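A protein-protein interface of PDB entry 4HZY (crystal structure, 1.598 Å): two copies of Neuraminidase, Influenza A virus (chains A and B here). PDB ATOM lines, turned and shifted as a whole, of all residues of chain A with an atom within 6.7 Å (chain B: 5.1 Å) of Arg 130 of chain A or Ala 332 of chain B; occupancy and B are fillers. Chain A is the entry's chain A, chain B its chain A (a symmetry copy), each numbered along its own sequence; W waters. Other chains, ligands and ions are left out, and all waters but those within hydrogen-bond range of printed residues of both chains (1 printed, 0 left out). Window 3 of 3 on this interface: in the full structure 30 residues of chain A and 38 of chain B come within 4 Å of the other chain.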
ATOM      1  N   ILE A 125      12.686 -18.660  -2.127  1.00  0.00           N
ATOM      2  CA  ILE A 125      11.919 -19.132  -3.270  1.00  0.00           C
ATOM      3  C   ILE A 125      10.635 -18.339  -3.309  1.00  0.00           C
ATOM      4  O   ILE A 125       9.881 -18.329  -2.330  1.00  0.00           O
ATOM      5  CB  ILE A 125      11.557 -20.628  -3.146  1.00  0.00           C
ATOM      6  CG1 ILE A 125      12.798 -21.480  -2.886  1.00  0.00           C
ATOM      7  CG2 ILE A 125      10.786 -21.107  -4.390  1.00  0.00           C
ATOM      8  CD1 ILE A 125      13.872 -21.372  -3.955  1.00  0.00           C
ATOM      9  N   ILE A 126      10.396 -17.671  -4.434  1.00  0.00           N
ATOM     10  CA  ILE A 126       9.197 -16.867  -4.635  1.00  0.00           C
ATOM     11  C   ILE A 126       8.351 -17.551  -5.691  1.00  0.00           C
ATOM     12  O   ILE A 126       8.865 -17.965  -6.733  1.00  0.00           O
ATOM     13  CB  ILE A 126       9.536 -15.453  -5.149  1.00  0.00           C
ATOM     14  CG1 ILE A 126      10.720 -14.852  -4.380  1.00  0.00           C
ATOM     15  CG2 ILE A 126       8.291 -14.555  -5.093  1.00  0.00           C
ATOM     16  CD1 ILE A 126      10.513 -14.819  -2.885  1.00  0.00           C
ATOM     17  N   TYR A 127       7.058 -17.701  -5.430  1.00  0.00           N
ATOM     18  CA  TYR A 127       6.184 -18.354  -6.395  1.00  0.00           C
ATOM     19  C   TYR A 127       4.874 -17.585  -6.454  1.00  0.00           C
ATOM     20  O   TYR A 127       4.202 -17.407  -5.443  1.00  0.00           O
ATOM     21  CB  TYR A 127       5.932 -19.829  -6.028  1.00  0.00           C
ATOM     22  CG  TYR A 127       5.090 -20.534  -7.068  1.00  0.00           C
ATOM     23  CD1 TYR A 127       5.659 -20.962  -8.267  1.00  0.00           C
ATOM     24  CD2 TYR A 127       3.732 -20.744  -6.870  1.00  0.00           C
ATOM     25  CE1 TYR A 127       4.905 -21.590  -9.243  1.00  0.00           C
ATOM     26  CE2 TYR A 127       2.964 -21.378  -7.838  1.00  0.00           C
ATOM     27  CZ  TYR A 127       3.555 -21.797  -9.022  1.00  0.00           C
ATOM     28  OH  TYR A 127       2.799 -22.425  -9.988  1.00  0.00           O
ATOM     29  N   GLY A 128       4.506 -17.126  -7.643  1.00  0.00           N
ATOM     30  CA  GLY A 128       3.340 -16.261  -7.762  1.00  0.00           C
ATOM     31  C   GLY A 128       3.406 -15.021  -6.883  1.00  0.00           C
ATOM     32  O   GLY A 128       2.375 -14.537  -6.409  1.00  0.00           O
ATOM     33  N   GLY A 129       4.613 -14.512  -6.654  1.00  0.00           N
ATOM     34  CA  GLY A 129       4.801 -13.302  -5.872  1.00  0.00           C
ATOM     35  C   GLY A 129       4.893 -13.514  -4.372  1.00  0.00           C
ATOM     36  O   GLY A 129       5.171 -12.566  -3.642  1.00  0.00           O
ATOM     37  N   ARG A 130       4.651 -14.737  -3.918  1.00  0.00           N
ATOM     38  CA  ARG A 130       4.711 -15.043  -2.494  1.00  0.00           C
ATOM     39  C   ARG A 130       5.974 -15.801  -2.162  1.00  0.00           C
ATOM     40  O   ARG A 130       6.369 -16.691  -2.901  1.00  0.00           O
ATOM     41  CB  ARG A 130       3.513 -15.893  -2.048  1.00  0.00           C
ATOM     42  CG  ARG A 130       3.522 -16.055  -0.532  1.00  0.00           C
ATOM     43  CD  ARG A 130       2.465 -16.981   0.048  1.00  0.00           C
ATOM     44  NE  ARG A 130       2.984 -17.498   1.307  1.00  0.00           N
ATOM     45  CZ  ARG A 130       3.476 -18.723   1.462  1.00  0.00           C
ATOM     46  NH1 ARG A 130       3.446 -19.582   0.453  1.00  0.00           N
ATOM     47  NH2 ARG A 130       3.954 -19.107   2.639  1.00  0.00           N
ATOM     48  N   MET A 131       6.602 -15.473  -1.038  1.00  0.00           N
ATOM     49  CA  MET A 131       7.733 -16.274  -0.583  1.00  0.00           C
ATOM     50  C   MET A 131       7.246 -17.603   0.004  1.00  0.00           C
ATOM     51  O   MET A 131       6.572 -17.628   1.035  1.00  0.00           O
ATOM     52  CB  MET A 131       8.566 -15.509   0.436  1.00  0.00           C
ATOM     53  CG  MET A 131       9.850 -16.243   0.788  1.00  0.00           C
ATOM     54  SD  MET A 131      10.710 -15.496   2.180  1.00  0.00           S
ATOM     55  CE  MET A 131      11.025 -13.831   1.587  1.00  0.00           C
ATOM     56  N   THR A 132       7.591 -18.702  -0.659  1.00  0.00           N
ATOM     57  CA  THR A 132       7.021 -20.009  -0.342  1.00  0.00           C
ATOM     58  C   THR A 132       8.004 -20.990   0.313  1.00  0.00           C
ATOM     59  O   THR A 132       7.585 -21.941   0.967  1.00  0.00           O
ATOM     60  CB  THR A 132       6.465 -20.681  -1.613  1.00  0.00           C
ATOM     61  OG1 THR A 132       7.470 -20.658  -2.631  1.00  0.00           O
ATOM     62  CG2 THR A 132       5.240 -19.949  -2.134  1.00  0.00           C
ATOM     63  N   ASP A 133       9.302 -20.780   0.135  1.00  0.00           N
ATOM     64  CA  ASP A 133      10.284 -21.714   0.692  1.00  0.00           C
ATOM     65  C   ASP A 133      11.656 -21.047   0.714  1.00  0.00           C
ATOM     66  O   ASP A 133      11.810 -19.895   0.290  1.00  0.00           O
ATOM     67  CB  ASP A 133      10.311 -23.007  -0.142  1.00  0.00           C
ATOM     68  CG  ASP A 133      10.533 -24.272   0.701  1.00  0.00           C
ATOM     69  OD1 ASP A 133      11.152 -24.185   1.782  1.00  0.00           O
ATOM     70  OD2 ASP A 133      10.090 -25.366   0.274  1.00  0.00           O
ATOM     71  N   GLU A 179       5.291 -25.626  -7.431  1.00  0.00           N
ATOM     72  CA  GLU A 179       4.442 -24.570  -6.890  1.00  0.00           C
ATOM     73  C   GLU A 179       5.104 -23.874  -5.706  1.00  0.00           C
ATOM     74  O   GLU A 179       4.450 -23.493  -4.731  1.00  0.00           O
ATOM     75  CB  GLU A 179       3.061 -25.118  -6.538  1.00  0.00           C
ATOM     76  CG  GLU A 179       2.354 -25.701  -7.759  1.00  0.00           C
ATOM     77  CD  GLU A 179       0.994 -26.305  -7.447  1.00  0.00           C
ATOM     78  OE1 GLU A 179       0.668 -26.498  -6.259  1.00  0.00           O
ATOM     79  OE2 GLU A 179       0.245 -26.590  -8.402  1.00  0.00           O
ATOM     80  N   GLY A 180       6.417 -23.705  -5.817  1.00  0.00           N
ATOM     81  CA  GLY A 180       7.175 -22.941  -4.849  1.00  0.00           C
ATOM     82  C   GLY A 180       7.636 -23.745  -3.649  1.00  0.00           C
ATOM     83  O   GLY A 180       8.304 -23.210  -2.777  1.00  0.00           O
ATOM     84  N   LYS A 181       7.294 -25.029  -3.604  1.00  0.00           N
ATOM     85  CA  LYS A 181       7.711 -25.869  -2.484  1.00  0.00           C
ATOM     86  C   LYS A 181       8.842 -26.788  -2.916  1.00  0.00           C
ATOM     87  O   LYS A 181       8.740 -27.471  -3.930  1.00  0.00           O
ATOM     88  CB  LYS A 181       6.529 -26.683  -1.950  1.00  0.00           C
ATOM     89  CG  LYS A 181       5.436 -25.807  -1.328  1.00  0.00           C
ATOM     90  CD  LYS A 181       6.061 -24.763  -0.391  1.00  0.00           C
ATOM     91  CE  LYS A 181       5.043 -23.754   0.125  1.00  0.00           C
ATOM     92  NZ  LYS A 181       4.016 -24.374   1.011  1.00  0.00           N
ATOM     93  N   CYS B  11       0.242 -19.080   9.456  1.00  0.00           N
ATOM     94  CA  CYS B  11       1.106 -20.193   9.089  1.00  0.00           C
ATOM     95  C   CYS B  11       2.164 -20.433  10.159  1.00  0.00           C
ATOM     96  O   CYS B  11       2.540 -19.527  10.892  1.00  0.00           O
ATOM     97  CB  CYS B  11       1.813 -19.896   7.766  1.00  0.00           C
ATOM     98  SG  CYS B  11       0.725 -19.614   6.342  1.00  0.00           S
ATOM     99  N   PHE B  19      12.790 -10.138   1.687  1.00  0.00           N
ATOM    100  CA  PHE B  19      11.771 -10.239   0.639  1.00  0.00           C
ATOM    101  C   PHE B  19      12.067  -9.176  -0.433  1.00  0.00           C
ATOM    102  O   PHE B  19      12.728  -9.466  -1.445  1.00  0.00           O
ATOM    103  CB  PHE B  19      10.403 -10.010   1.310  1.00  0.00           C
ATOM    104  CG  PHE B  19       9.194 -10.380   0.483  1.00  0.00           C
ATOM    105  CD1 PHE B  19       9.259 -11.249  -0.589  1.00  0.00           C
ATOM    106  CD2 PHE B  19       7.960  -9.830   0.815  1.00  0.00           C
ATOM    107  CE1 PHE B  19       8.092 -11.576  -1.313  1.00  0.00           C
ATOM    108  CE2 PHE B  19       6.810 -10.150   0.098  1.00  0.00           C
ATOM    109  CZ  PHE B  19       6.880 -11.022  -0.960  1.00  0.00           C
ATOM    110  N   VAL B 330       0.202 -12.387   3.891  1.00  0.00           N
ATOM    111  CA  VAL B 330       0.060 -12.855   2.523  1.00  0.00           C
ATOM    112  C   VAL B 330      -0.640 -14.206   2.575  1.00  0.00           C
ATOM    113  O   VAL B 330      -0.227 -15.084   3.338  1.00  0.00           O
ATOM    114  CB  VAL B 330       1.441 -12.998   1.854  1.00  0.00           C
ATOM    115  CG1 VAL B 330       1.281 -13.464   0.413  1.00  0.00           C
ATOM    116  CG2 VAL B 330       2.219 -11.671   1.912  1.00  0.00           C
ATOM    117  N   LYS B 331      -1.715 -14.379   1.806  1.00  0.00           N
ATOM    118  CA  LYS B 331      -2.435 -15.649   1.856  1.00  0.00           C
ATOM    119  C   LYS B 331      -1.579 -16.760   1.276  1.00  0.00           C
ATOM    120  O   LYS B 331      -1.007 -16.612   0.197  1.00  0.00           O
ATOM    121  CB  LYS B 331      -3.758 -15.580   1.096  1.00  0.00           C
ATOM    122  CG  LYS B 331      -4.543 -16.881   1.175  1.00  0.00           C
ATOM    123  CD  LYS B 331      -5.828 -16.819   0.372  1.00  0.00           C
ATOM    124  CE  LYS B 331      -6.547 -18.153   0.436  1.00  0.00           C
ATOM    125  NZ  LYS B 331      -7.739 -18.187  -0.454  1.00  0.00           N
ATOM    126  N   ALA B 332      -1.469 -17.856   2.014  1.00  0.00           N
ATOM    127  CA  ALA B 332      -0.836 -19.062   1.509  1.00  0.00           C
ATOM    128  C   ALA B 332      -1.949 -20.057   1.186  1.00  0.00           C
ATOM    129  O   ALA B 332      -3.032 -19.652   0.780  1.00  0.00           O
ATOM    130  CB  ALA B 332       0.149 -19.617   2.524  1.00  0.00           C
ATOM    131  N   LYS B 333      -1.706 -21.349   1.342  1.00  0.00           N
ATOM    132  CA  LYS B 333      -2.731 -22.311   0.945  1.00  0.00           C
ATOM    133  C   LYS B 333      -3.969 -22.210   1.839  1.00  0.00           C
ATOM    134  O   LYS B 333      -5.041 -21.811   1.385  1.00  0.00           O
ATOM    135  CB  LYS B 333      -2.161 -23.733   0.899  1.00  0.00           C
ATOM    136  CG  LYS B 333      -1.252 -23.958  -0.308  1.00  0.00           C
ATOM    137  CD  LYS B 333      -0.088 -24.897  -0.013  1.00  0.00           C
ATOM    138  CE  LYS B 333      -0.477 -26.357  -0.190  1.00  0.00           C
ATOM    139  NZ  LYS B 333       0.576 -27.115  -0.931  1.00  0.00           N
ATOM    140  N   ASP B 334      -3.802 -22.544   3.115  1.00  0.00           N
ATOM    141  CA  ASP B 334      -4.895 -22.504   4.080  1.00  0.00           C
ATOM    142  C   ASP B 334      -4.479 -21.756   5.346  1.00  0.00           C
ATOM    143  O   ASP B 334      -4.980 -22.021   6.439  1.00  0.00           O
ATOM    144  CB  ASP B 334      -5.351 -23.923   4.424  1.00  0.00           C
ATOM    145  CG  ASP B 334      -4.232 -24.933   4.309  1.00  0.00           C
ATOM    146  OD1 ASP B 334      -4.506 -26.074   3.871  1.00  0.00           O
ATOM    147  OD2 ASP B 334      -3.079 -24.585   4.647  1.00  0.00           O
ATOM    148  N   CYS B 335      -3.550 -20.820   5.191  1.00  0.00           N
ATOM    149  CA  CYS B 335      -3.101 -20.017   6.314  1.00  0.00           C
ATOM    150  C   CYS B 335      -2.589 -18.693   5.783  1.00  0.00           C
ATOM    151  O   CYS B 335      -2.419 -18.538   4.574  1.00  0.00           O
ATOM    152  CB  CYS B 335      -2.015 -20.739   7.116  1.00  0.00           C
ATOM    153  SG  CYS B 335      -0.523 -21.225   6.186  1.00  0.00           S
ATOM    154  N   PHE B 336      -2.395 -17.734   6.686  1.00  0.00           N
ATOM    155  CA  PHE B 336      -1.807 -16.445   6.342  1.00  0.00           C
ATOM    156  C   PHE B 336      -0.343 -16.427   6.753  1.00  0.00           C
ATOM    157  O   PHE B 336      -0.009 -16.776   7.874  1.00  0.00           O
ATOM    158  CB  PHE B 336      -2.541 -15.303   7.057  1.00  0.00           C
ATOM    159  CG  PHE B 336      -3.859 -14.956   6.444  1.00  0.00           C
ATOM    160  CD1 PHE B 336      -3.939 -14.579   5.113  1.00  0.00           C
ATOM    161  CD2 PHE B 336      -5.015 -14.968   7.204  1.00  0.00           C
ATOM    162  CE1 PHE B 336      -5.155 -14.250   4.538  1.00  0.00           C
ATOM    163  CE2 PHE B 336      -6.239 -14.641   6.639  1.00  0.00           C
ATOM    164  CZ  PHE B 336      -6.312 -14.282   5.303  1.00  0.00           C
ATOM    165  N   GLN B 337       0.526 -16.010   5.839  1.00  0.00           N
ATOM    166  CA  GLN B 337       1.938 -15.906   6.142  1.00  0.00           C
ATOM    167  C   GLN B 337       2.222 -14.545   6.766  1.00  0.00           C
ATOM    168  O   GLN B 337       1.807 -13.514   6.219  1.00  0.00           O
ATOM    169  CB  GLN B 337       2.729 -16.036   4.851  1.00  0.00           C
ATOM    170  CG  GLN B 337       4.209 -15.752   4.995  1.00  0.00           C
ATOM    171  CD  GLN B 337       4.899 -15.875   3.668  1.00  0.00           C
ATOM    172  OE1 GLN B 337       4.338 -15.506   2.634  1.00  0.00           O
ATOM    173  NE2 GLN B 337       6.105 -16.435   3.673  1.00  0.00           N
ATOM    174  N   LEU B 368       8.925 -17.962   7.356  1.00  0.00           N
ATOM    175  CA  LEU B 368       8.841 -19.324   6.842  1.00  0.00           C
ATOM    176  C   LEU B 368       9.168 -20.298   7.963  1.00  0.00           C
ATOM    177  O   LEU B 368       9.843 -19.934   8.924  1.00  0.00           O
ATOM    178  CB  LEU B 368       9.841 -19.566   5.715  1.00  0.00           C
ATOM    179  CG  LEU B 368       9.684 -18.739   4.443  1.00  0.00           C
ATOM    180  CD1 LEU B 368      10.932 -18.923   3.599  1.00  0.00           C
ATOM    181  CD2 LEU B 368       8.413 -19.138   3.683  1.00  0.00           C
HETATM  182  O   HOH W   1       5.381 -13.727   0.818  1.00  0.00           O
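The guanidinium group of Arg 130 of chain A lies within hydrogen-bond range of the side-chain amide oxygen of Gln 337 of chain B (2.7 Å). NE2 of Gln 337 of chain B is in hydrogen-bond range of O of Met 131 of chain A (2.9 Å).
N of Ile 125 of chain A sits at hydrogen-bond distance from O of Asp 133 of chain A, at 2.9 Å. The backbone NH of Gln 337 of chain B sits at hydrogen-bond distance from the backbone carbonyl oxygen of Val 330 of chain B, at 2.8 Å. SG of Cys 11 of chain B forms a disulfide with SG of Cys 335 of chain B (2.0 Å). N of Thr 132 of chain A lies within hydrogen-bond range of O of Ile 125 of chain A (2.9 Å). SG of Cys 11 of chain B sits at hydrogen-bond distance from N of Gln 337 of chain B (3.6 Å). The side-chain hydroxyl (OG1) of Thr 132 of chain A lies within hydrogen-bond range of the backbone carbonyl oxygen (O) of Gly 180 of chain A, at 2.7 Å.
CZ of Phe 19 of chain B touches O of Gly 129 of chain A (3.5 Å). Arg 130 of chain A touches Val 330 of chain B (CG to CG1, 3.6 Å). Arg 130 of chain A touches Lys 331 of chain B. Ala 332 of chain B touches Arg 130 of chain A. Phe 19 of chain B touches Met 131 of chain A. CD2 of Leu 368 of chain B touches O of Met 131 of chain A, 3.6 Å away. CD2 of Leu 368 of chain B touches C of Thr 132 of chain A, at 3.9 Å. Asp 133 of chain A touches Leu 368 of chain B.
Of the printed residues of chain B, Met 131 of chain A touches Phe 19 (3.8 Å), Gln 337 (2.9 Å) and Leu 368 (3.6 Å). Of the printed residues of chain A, Phe 19 of chain B touches Gly 129 and Met 131. Of the printed residues of chain A, Val 330 of chain B touches Arg 130 (3.6 Å). Of the printed residues of chain A, Ala 332 of chain B touches Arg 130. Of the printed residues of chain A, Leu 368 of chain B touches Met 131 (3.6 Å), Thr 132 (3.9 Å) and Asp 133 (3.6 Å). The nearest residue of chain B that does not touch Arg 130 of chain A is Leu 368 of chain B (4.6 Å). The nearest printed residue of chain A that does not touch Gln 337 of chain B is Thr 132 of chain A (5.1 Å).
Hydrophobic or aromatic side chains of chain A that line the printed part of chain B: Met 131. Hydrophobic or aromatic side chains of chain B that line the printed part of chain A: Phe 19, Val 330, Ala 332 and Leu 368. Among the printed residues, no Asp or Glu carboxylate lies within 4 Å of a Lys or Arg side-chain nitrogen of the other chain.
No position is printed for both chains.
Water W1 bridges the side-chain amide oxygen of Gln 337 of chain B (2.7 Å) and the backbone NH of Met 131 of chain A (2.8 Å).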
